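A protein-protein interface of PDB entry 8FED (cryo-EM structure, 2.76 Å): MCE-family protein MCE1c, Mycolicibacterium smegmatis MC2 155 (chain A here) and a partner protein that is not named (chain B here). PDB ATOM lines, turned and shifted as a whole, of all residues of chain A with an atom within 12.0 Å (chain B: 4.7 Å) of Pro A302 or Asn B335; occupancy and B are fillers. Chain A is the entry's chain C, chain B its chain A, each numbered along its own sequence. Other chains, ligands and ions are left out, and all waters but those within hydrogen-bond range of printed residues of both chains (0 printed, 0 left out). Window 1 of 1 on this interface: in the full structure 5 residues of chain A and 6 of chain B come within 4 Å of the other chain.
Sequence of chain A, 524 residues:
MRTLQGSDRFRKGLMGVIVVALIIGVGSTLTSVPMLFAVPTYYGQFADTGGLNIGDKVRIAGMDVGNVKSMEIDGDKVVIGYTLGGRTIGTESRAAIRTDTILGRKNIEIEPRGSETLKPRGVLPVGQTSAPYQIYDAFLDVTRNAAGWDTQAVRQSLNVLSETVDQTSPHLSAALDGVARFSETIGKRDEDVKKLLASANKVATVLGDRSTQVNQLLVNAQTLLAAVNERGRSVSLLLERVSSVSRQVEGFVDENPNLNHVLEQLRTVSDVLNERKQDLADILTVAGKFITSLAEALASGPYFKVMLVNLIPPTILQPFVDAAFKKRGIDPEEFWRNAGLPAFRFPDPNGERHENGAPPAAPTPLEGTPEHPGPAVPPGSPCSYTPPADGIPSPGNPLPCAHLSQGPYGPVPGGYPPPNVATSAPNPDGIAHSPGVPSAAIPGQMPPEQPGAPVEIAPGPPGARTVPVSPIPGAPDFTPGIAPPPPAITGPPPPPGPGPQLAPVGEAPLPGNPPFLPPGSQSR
N of Tyr B337 sits close to O of Ser A300 (3.4 Å).
OH of Tyr B383 sits at hydrogen-bond distance from N of Asn B335. ND2 of Asn B335 lies close to N of Gln B390 (3.2 Å). The side-chain hydroxyl of Ser A300 lies close to the side-chain amino group of Lys A305, at 3.3 Å.
Ala A299 touches Tyr B337. Pro B336 touches Ser A300. Gly A301 touches Tyr B337 (CA to CE2, 3.4 Å). Pro A302 touches Asn B335 (CD to O, 3.8 Å). Pro A302 touches Tyr B337. CB of Pro A302 touches CG2 of Ile B380, at 3.8 Å. Val B333 touches Tyr A303. Gly B334 touches Tyr A303. Tyr A303 touches Pro B336 (OH to CG, 3.4 Å).
Pro A302 touches three residues of chain B. Of chain A, only Pro A302 (3.8 Å) comes within 4 Å of Asn B335. Of chain A, only Tyr A303 (3.6 Å) comes within 4 Å of Val B333. Of chain A, only Tyr A303 comes within 4 Å of Gly B334. Pro B336 touches two residues of chain A. No residue of chain A comes within 4 Å of Gly B389. Gln B390 touches none of the printed residues of chain A. No residue of chain A comes within 4 Å of Pro B391. No residue of chain A comes within 4 Å of Pro B409. Printed residues of chain B within 4 Å of Ser A300: Pro B336 (3.8 Å) and Tyr B337 (3.1 Å). Of the printed residues of chain B, Gly A301 touches Tyr B337. Of the printed residues of chain B, Tyr A303 touches Val B333, Gly B334 and Pro B336. Printed residues of chain B within 4 Å of Ala A299: Tyr B337. Ala A295 touches none of the printed residues of chain B. Lys A305 touches none of the printed residues of chain B.
Printed residues of chain A that touch a printed residue of chain B: Ala A299, Ser A300, Gly A301, Pro A302 and Tyr A303. Hydrophobic or aromatic side chains of chain A that line the printed part of chain B: Pro A302 and Tyr A303. Along chain A the printed residues that touch a printed residue of chain B span positions 299 to 303. Of the 11 printed residues of chain B, 6 touch a printed residue of chain A. Among the printed residues, 10 pairs touch across the chains.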
ATOM      1  N   ALA A 295      12.702  28.438 -12.957  1.00  0.00           N
ATOM      2  CA  ALA A 295      12.335  27.315 -13.810  1.00  0.00           C
ATOM      3  C   ALA A 295      10.854  27.286 -14.153  1.00  0.00           C
ATOM      4  O   ALA A 295      10.457  26.502 -15.020  1.00  0.00           O
ATOM      5  CB  ALA A 295      12.720  25.995 -13.146  1.00  0.00           C
ATOM      6  N   GLU A 296      10.029  28.084 -13.470  1.00  0.00           N
ATOM      7  CA  GLU A 296       8.612  28.125 -13.812  1.00  0.00           C
ATOM      8  C   GLU A 296       8.377  28.659 -15.218  1.00  0.00           C
ATOM      9  O   GLU A 296       7.536  28.126 -15.953  1.00  0.00           O
ATOM     10  CB  GLU A 296       7.858  28.976 -12.791  1.00  0.00           C
ATOM     11  CG  GLU A 296       6.433  28.522 -12.564  1.00  0.00           C
ATOM     12  CD  GLU A 296       6.368  27.123 -11.991  1.00  0.00           C
ATOM     13  OE1 GLU A 296       7.288  26.755 -11.235  1.00  0.00           O
ATOM     14  OE2 GLU A 296       5.412  26.386 -12.303  1.00  0.00           O
ATOM     15  N   ALA A 297       9.102  29.712 -15.612  1.00  0.00           N
ATOM     16  CA  ALA A 297       8.805  30.386 -16.876  1.00  0.00           C
ATOM     17  C   ALA A 297       8.984  29.451 -18.062  1.00  0.00           C
ATOM     18  O   ALA A 297       8.151  29.415 -18.973  1.00  0.00           O
ATOM     19  CB  ALA A 297       9.687  31.623 -17.033  1.00  0.00           C
ATOM     20  N   LEU A 298      10.066  28.684 -18.059  1.00  0.00           N
ATOM     21  CA  LEU A 298      10.380  27.726 -19.115  1.00  0.00           C
ATOM     22  C   LEU A 298       9.828  26.328 -18.807  1.00  0.00           C
ATOM     23  O   LEU A 298      10.526  25.319 -18.776  1.00  0.00           O
ATOM     24  CB  LEU A 298      11.886  27.778 -19.368  1.00  0.00           C
ATOM     25  CG  LEU A 298      12.995  27.470 -18.344  1.00  0.00           C
ATOM     26  CD1 LEU A 298      13.355  26.033 -18.063  1.00  0.00           C
ATOM     27  CD2 LEU A 298      14.228  28.270 -18.728  1.00  0.00           C
ATOM     28  N   ALA A 299       8.506  26.280 -18.641  1.00  0.00           N
ATOM     29  CA  ALA A 299       7.815  25.041 -18.298  1.00  0.00           C
ATOM     30  C   ALA A 299       6.645  24.753 -19.233  1.00  0.00           C
ATOM     31  O   ALA A 299       6.296  23.589 -19.454  1.00  0.00           O
ATOM     32  CB  ALA A 299       7.322  25.087 -16.851  1.00  0.00           C
ATOM     33  N   SER A 300       6.034  25.808 -19.780  1.00  0.00           N
ATOM     34  CA  SER A 300       4.831  25.649 -20.595  1.00  0.00           C
ATOM     35  C   SER A 300       5.107  24.849 -21.862  1.00  0.00           C
ATOM     36  O   SER A 300       4.334  23.956 -22.222  1.00  0.00           O
ATOM     37  CB  SER A 300       4.250  27.020 -20.942  1.00  0.00           C
ATOM     38  OG  SER A 300       3.880  27.730 -19.775  1.00  0.00           O
ATOM     39  N   GLY A 301       6.203  25.155 -22.554  1.00  0.00           N
ATOM     40  CA  GLY A 301       6.517  24.484 -23.794  1.00  0.00           C
ATOM     41  C   GLY A 301       8.006  24.406 -24.052  1.00  0.00           C
ATOM     42  O   GLY A 301       8.826  24.714 -23.180  1.00  0.00           O
ATOM     43  N   PRO A 302       8.393  23.981 -25.261  1.00  0.00           N
ATOM     44  CA  PRO A 302       9.817  23.990 -25.651  1.00  0.00           C
ATOM     45  C   PRO A 302      10.313  25.389 -26.003  1.00  0.00           C
ATOM     46  O   PRO A 302      10.778  25.655 -27.114  1.00  0.00           O
ATOM     47  CB  PRO A 302       9.833  23.036 -26.851  1.00  0.00           C
ATOM     48  CG  PRO A 302       8.480  23.149 -27.432  1.00  0.00           C
ATOM     49  CD  PRO A 302       7.547  23.331 -26.274  1.00  0.00           C
ATOM     50  N   TYR A 303      10.214  26.293 -25.039  1.00  0.00           N
ATOM     51  CA  TYR A 303      10.590  27.697 -25.180  1.00  0.00           C
ATOM     52  C   TYR A 303      10.602  28.301 -23.779  1.00  0.00           C
ATOM     53  O   TYR A 303      10.438  27.590 -22.781  1.00  0.00           O
ATOM     54  CB  TYR A 303       9.641  28.440 -26.122  1.00  0.00           C
ATOM     55  CG  TYR A 303       8.222  27.913 -26.114  1.00  0.00           C
ATOM     56  CD1 TYR A 303       7.356  28.196 -25.066  1.00  0.00           C
ATOM     57  CD2 TYR A 303       7.748  27.134 -27.160  1.00  0.00           C
ATOM     58  CE1 TYR A 303       6.061  27.715 -25.062  1.00  0.00           C
ATOM     59  CE2 TYR A 303       6.458  26.648 -27.161  1.00  0.00           C
ATOM     60  CZ  TYR A 303       5.620  26.941 -26.113  1.00  0.00           C
ATOM     61  OH  TYR A 303       4.337  26.455 -26.121  1.00  0.00           O
ATOM     62  N   PHE A 304      10.800  29.613 -23.698  1.00  0.00           N
ATOM     63  CA  PHE A 304      10.692  30.329 -22.435  1.00  0.00           C
ATOM     64  C   PHE A 304      10.051  31.684 -22.684  1.00  0.00           C
ATOM     65  O   PHE A 304      10.417  32.381 -23.632  1.00  0.00           O
ATOM     66  CB  PHE A 304      12.064  30.487 -21.762  1.00  0.00           C
ATOM     67  CG  PHE A 304      13.036  31.334 -22.533  1.00  0.00           C
ATOM     68  CD1 PHE A 304      13.766  30.797 -23.576  1.00  0.00           C
ATOM     69  CD2 PHE A 304      13.240  32.662 -22.197  1.00  0.00           C
ATOM     70  CE1 PHE A 304      14.661  31.570 -24.281  1.00  0.00           C
ATOM     71  CE2 PHE A 304      14.138  33.437 -22.898  1.00  0.00           C
ATOM     72  CZ  PHE A 304      14.846  32.892 -23.941  1.00  0.00           C
ATOM     73  N   LYS A 305       9.094  32.051 -21.841  1.00  0.00           N
ATOM     74  CA  LYS A 305       8.385  33.305 -22.033  1.00  0.00           C
ATOM     75  C   LYS A 305       9.266  34.489 -21.659  1.00  0.00           C
ATOM     76  O   LYS A 305      10.148  34.391 -20.802  1.00  0.00           O
ATOM     77  CB  LYS A 305       7.102  33.319 -21.211  1.00  0.00           C
ATOM     78  CG  LYS A 305       6.218  32.112 -21.453  1.00  0.00           C
ATOM     79  CD  LYS A 305       4.925  32.208 -20.674  1.00  0.00           C
ATOM     80  CE  LYS A 305       4.252  30.857 -20.598  1.00  0.00           C
ATOM     81  NZ  LYS A 305       4.221  30.215 -21.934  1.00  0.00           N
ATOM     82  N   VAL A 306       9.021  35.619 -22.318  1.00  0.00           N
ATOM     83  CA  VAL A 306       9.744  36.862 -22.067  1.00  0.00           C
ATOM     84  C   VAL A 306       8.760  38.020 -22.129  1.00  0.00           C
ATOM     85  O   VAL A 306       7.821  38.008 -22.929  1.00  0.00           O
ATOM     86  CB  VAL A 306      10.893  37.079 -23.073  1.00  0.00           C
ATOM     87  CG1 VAL A 306      12.062  36.182 -22.748  1.00  0.00           C
ATOM     88  CG2 VAL A 306      10.415  36.825 -24.489  1.00  0.00           C
ATOM     89  N   VAL B 333       7.084  27.773 -33.060  1.00  0.00           N
ATOM     90  CA  VAL B 333       7.244  27.039 -31.813  1.00  0.00           C
ATOM     91  C   VAL B 333       6.353  25.805 -31.836  1.00  0.00           C
ATOM     92  O   VAL B 333       5.342  25.746 -32.538  1.00  0.00           O
ATOM     93  CB  VAL B 333       6.923  27.909 -30.585  1.00  0.00           C
ATOM     94  CG1 VAL B 333       8.046  28.885 -30.335  1.00  0.00           C
ATOM     95  CG2 VAL B 333       5.612  28.645 -30.790  1.00  0.00           C
ATOM     96  N   GLY B 334       6.740  24.813 -31.035  1.00  0.00           N
ATOM     97  CA  GLY B 334       6.049  23.545 -31.010  1.00  0.00           C
ATOM     98  C   GLY B 334       4.843  23.543 -30.094  1.00  0.00           C
ATOM     99  O   GLY B 334       4.517  24.523 -29.425  1.00  0.00           O
ATOM    100  N   ASN B 335       4.166  22.400 -30.075  1.00  0.00           N
ATOM    101  CA  ASN B 335       2.967  22.253 -29.265  1.00  0.00           C
ATOM    102  C   ASN B 335       3.327  22.237 -27.781  1.00  0.00           C
ATOM    103  O   ASN B 335       4.306  21.594 -27.387  1.00  0.00           O
ATOM    104  CB  ASN B 335       2.228  20.968 -29.631  1.00  0.00           C
ATOM    105  CG  ASN B 335       2.102  20.775 -31.123  1.00  0.00           C
ATOM    106  OD1 ASN B 335       2.452  19.723 -31.655  1.00  0.00           O
ATOM    107  ND2 ASN B 335       1.602  21.794 -31.811  1.00  0.00           N
ATOM    108  N   PRO B 336       2.563  22.934 -26.940  1.00  0.00           N
ATOM    109  CA  PRO B 336       2.790  22.851 -25.494  1.00  0.00           C
ATOM    110  C   PRO B 336       2.613  21.429 -24.982  1.00  0.00           C
ATOM    111  O   PRO B 336       2.018  20.570 -25.637  1.00  0.00           O
ATOM    112  CB  PRO B 336       1.724  23.787 -24.913  1.00  0.00           C
ATOM    113  CG  PRO B 336       1.425  24.740 -26.013  1.00  0.00           C
ATOM    114  CD  PRO B 336       1.550  23.946 -27.281  1.00  0.00           C
ATOM    115  N   TYR B 337       3.153  21.183 -23.793  1.00  0.00           N
ATOM    116  CA  TYR B 337       3.097  19.848 -23.219  1.00  0.00           C
ATOM    117  C   TYR B 337       1.672  19.485 -22.821  1.00  0.00           C
ATOM    118  O   TYR B 337       0.914  20.323 -22.325  1.00  0.00           O
ATOM    119  CB  TYR B 337       4.013  19.751 -22.002  1.00  0.00           C
ATOM    120  CG  TYR B 337       5.452  20.124 -22.268  1.00  0.00           C
ATOM    121  CD1 TYR B 337       6.308  19.252 -22.922  1.00  0.00           C
ATOM    122  CD2 TYR B 337       5.965  21.333 -21.828  1.00  0.00           C
ATOM    123  CE1 TYR B 337       7.626  19.589 -23.158  1.00  0.00           C
ATOM    124  CE2 TYR B 337       7.281  21.672 -22.052  1.00  0.00           C
ATOM    125  CZ  TYR B 337       8.105  20.802 -22.719  1.00  0.00           C
ATOM    126  OH  TYR B 337       9.416  21.150 -22.943  1.00  0.00           O
ATOM    127  N   ILE B 380      11.926  16.998 -28.203  1.00  0.00           N
ATOM    128  CA  ILE B 380      11.576  17.675 -29.447  1.00  0.00           C
ATOM    129  C   ILE B 380      12.108  16.856 -30.616  1.00  0.00           C
ATOM    130  O   ILE B 380      12.410  17.395 -31.685  1.00  0.00           O
ATOM    131  CB  ILE B 380      12.108  19.120 -29.483  1.00  0.00           C
ATOM    132  CG1 ILE B 380      13.630  19.146 -29.353  1.00  0.00           C
ATOM    133  CG2 ILE B 380      11.462  19.956 -28.391  1.00  0.00           C
ATOM    134  CD1 ILE B 380      14.207  20.537 -29.377  1.00  0.00           C
ATOM    135  N   TYR B 383      10.118  16.750 -34.336  1.00  0.00           N
ATOM    136  CA  TYR B 383       9.956  18.017 -35.046  1.00  0.00           C
ATOM    137  C   TYR B 383      10.876  18.058 -36.270  1.00  0.00           C
ATOM    138  O   TYR B 383      11.793  18.869 -36.377  1.00  0.00           O
ATOM    139  CB  TYR B 383      10.225  19.188 -34.113  1.00  0.00           C
ATOM    140  CG  TYR B 383       9.132  19.438 -33.103  1.00  0.00           C
ATOM    141  CD1 TYR B 383       8.067  20.273 -33.401  1.00  0.00           C
ATOM    142  CD2 TYR B 383       9.169  18.847 -31.847  1.00  0.00           C
ATOM    143  CE1 TYR B 383       7.067  20.510 -32.483  1.00  0.00           C
ATOM    144  CE2 TYR B 383       8.173  19.080 -30.920  1.00  0.00           C
ATOM    145  CZ  TYR B 383       7.125  19.912 -31.243  1.00  0.00           C
ATOM    146  OH  TYR B 383       6.130  20.146 -30.325  1.00  0.00           O
ATOM    147  N   GLY B 389       0.303  24.143 -36.080  1.00  0.00           N
ATOM    148  CA  GLY B 389       0.149  23.853 -34.667  1.00  0.00           C
ATOM    149  C   GLY B 389      -1.150  23.156 -34.322  1.00  0.00           C
ATOM    150  O   GLY B 389      -2.218  23.562 -34.792  1.00  0.00           O
ATOM    151  N   GLN B 390      -1.070  22.094 -33.518  1.00  0.00           N
ATOM    152  CA  GLN B 390      -2.278  21.369 -33.128  1.00  0.00           C
ATOM    153  C   GLN B 390      -3.263  22.255 -32.369  1.00  0.00           C
ATOM    154  O   GLN B 390      -4.458  22.233 -32.709  1.00  0.00           O
ATOM    155  CB  GLN B 390      -1.897  20.108 -32.344  1.00  0.00           C
ATOM    156  CG  GLN B 390      -0.855  19.239 -33.026  1.00  0.00           C
ATOM    157  CD  GLN B 390      -1.330  18.674 -34.347  1.00  0.00           C
ATOM    158  OE1 GLN B 390      -2.529  18.504 -34.571  1.00  0.00           O
ATOM    159  NE2 GLN B 390      -0.389  18.381 -35.236  1.00  0.00           N
ATOM    160  N   PRO B 391      -2.858  23.047 -31.353  1.00  0.00           N
ATOM    161  CA  PRO B 391      -3.798  24.072 -30.845  1.00  0.00           C
ATOM    162  C   PRO B 391      -3.664  25.373 -31.631  1.00  0.00           C
ATOM    163  O   PRO B 391      -3.184  26.399 -31.131  1.00  0.00           O
ATOM    164  CB  PRO B 391      -3.371  24.222 -29.379  1.00  0.00           C
ATOM    165  CG  PRO B 391      -2.305  23.184 -29.134  1.00  0.00           C
ATOM    166  CD  PRO B 391      -1.696  22.930 -30.460  1.00  0.00           C
ATOM    167  N   PRO B 409       3.403  14.905 -33.222  1.00  0.00           N
ATOM    168  CA  PRO B 409       3.077  15.822 -34.315  1.00  0.00           C
ATOM    169  C   PRO B 409       3.774  15.428 -35.613  1.00  0.00           C
ATOM    170  O   PRO B 409       4.780  14.720 -35.596  1.00  0.00           O
ATOM    171  CB  PRO B 409       3.589  17.167 -33.803  1.00  0.00           C
ATOM    172  CG  PRO B 409       4.727  16.811 -32.929  1.00  0.00           C
ATOM    173  CD  PRO B 409       4.385  15.492 -32.292  1.00  0.00           C
ATOM    174  OXT PRO B 409       3.345  15.795 -36.705  1.00  0.00           O
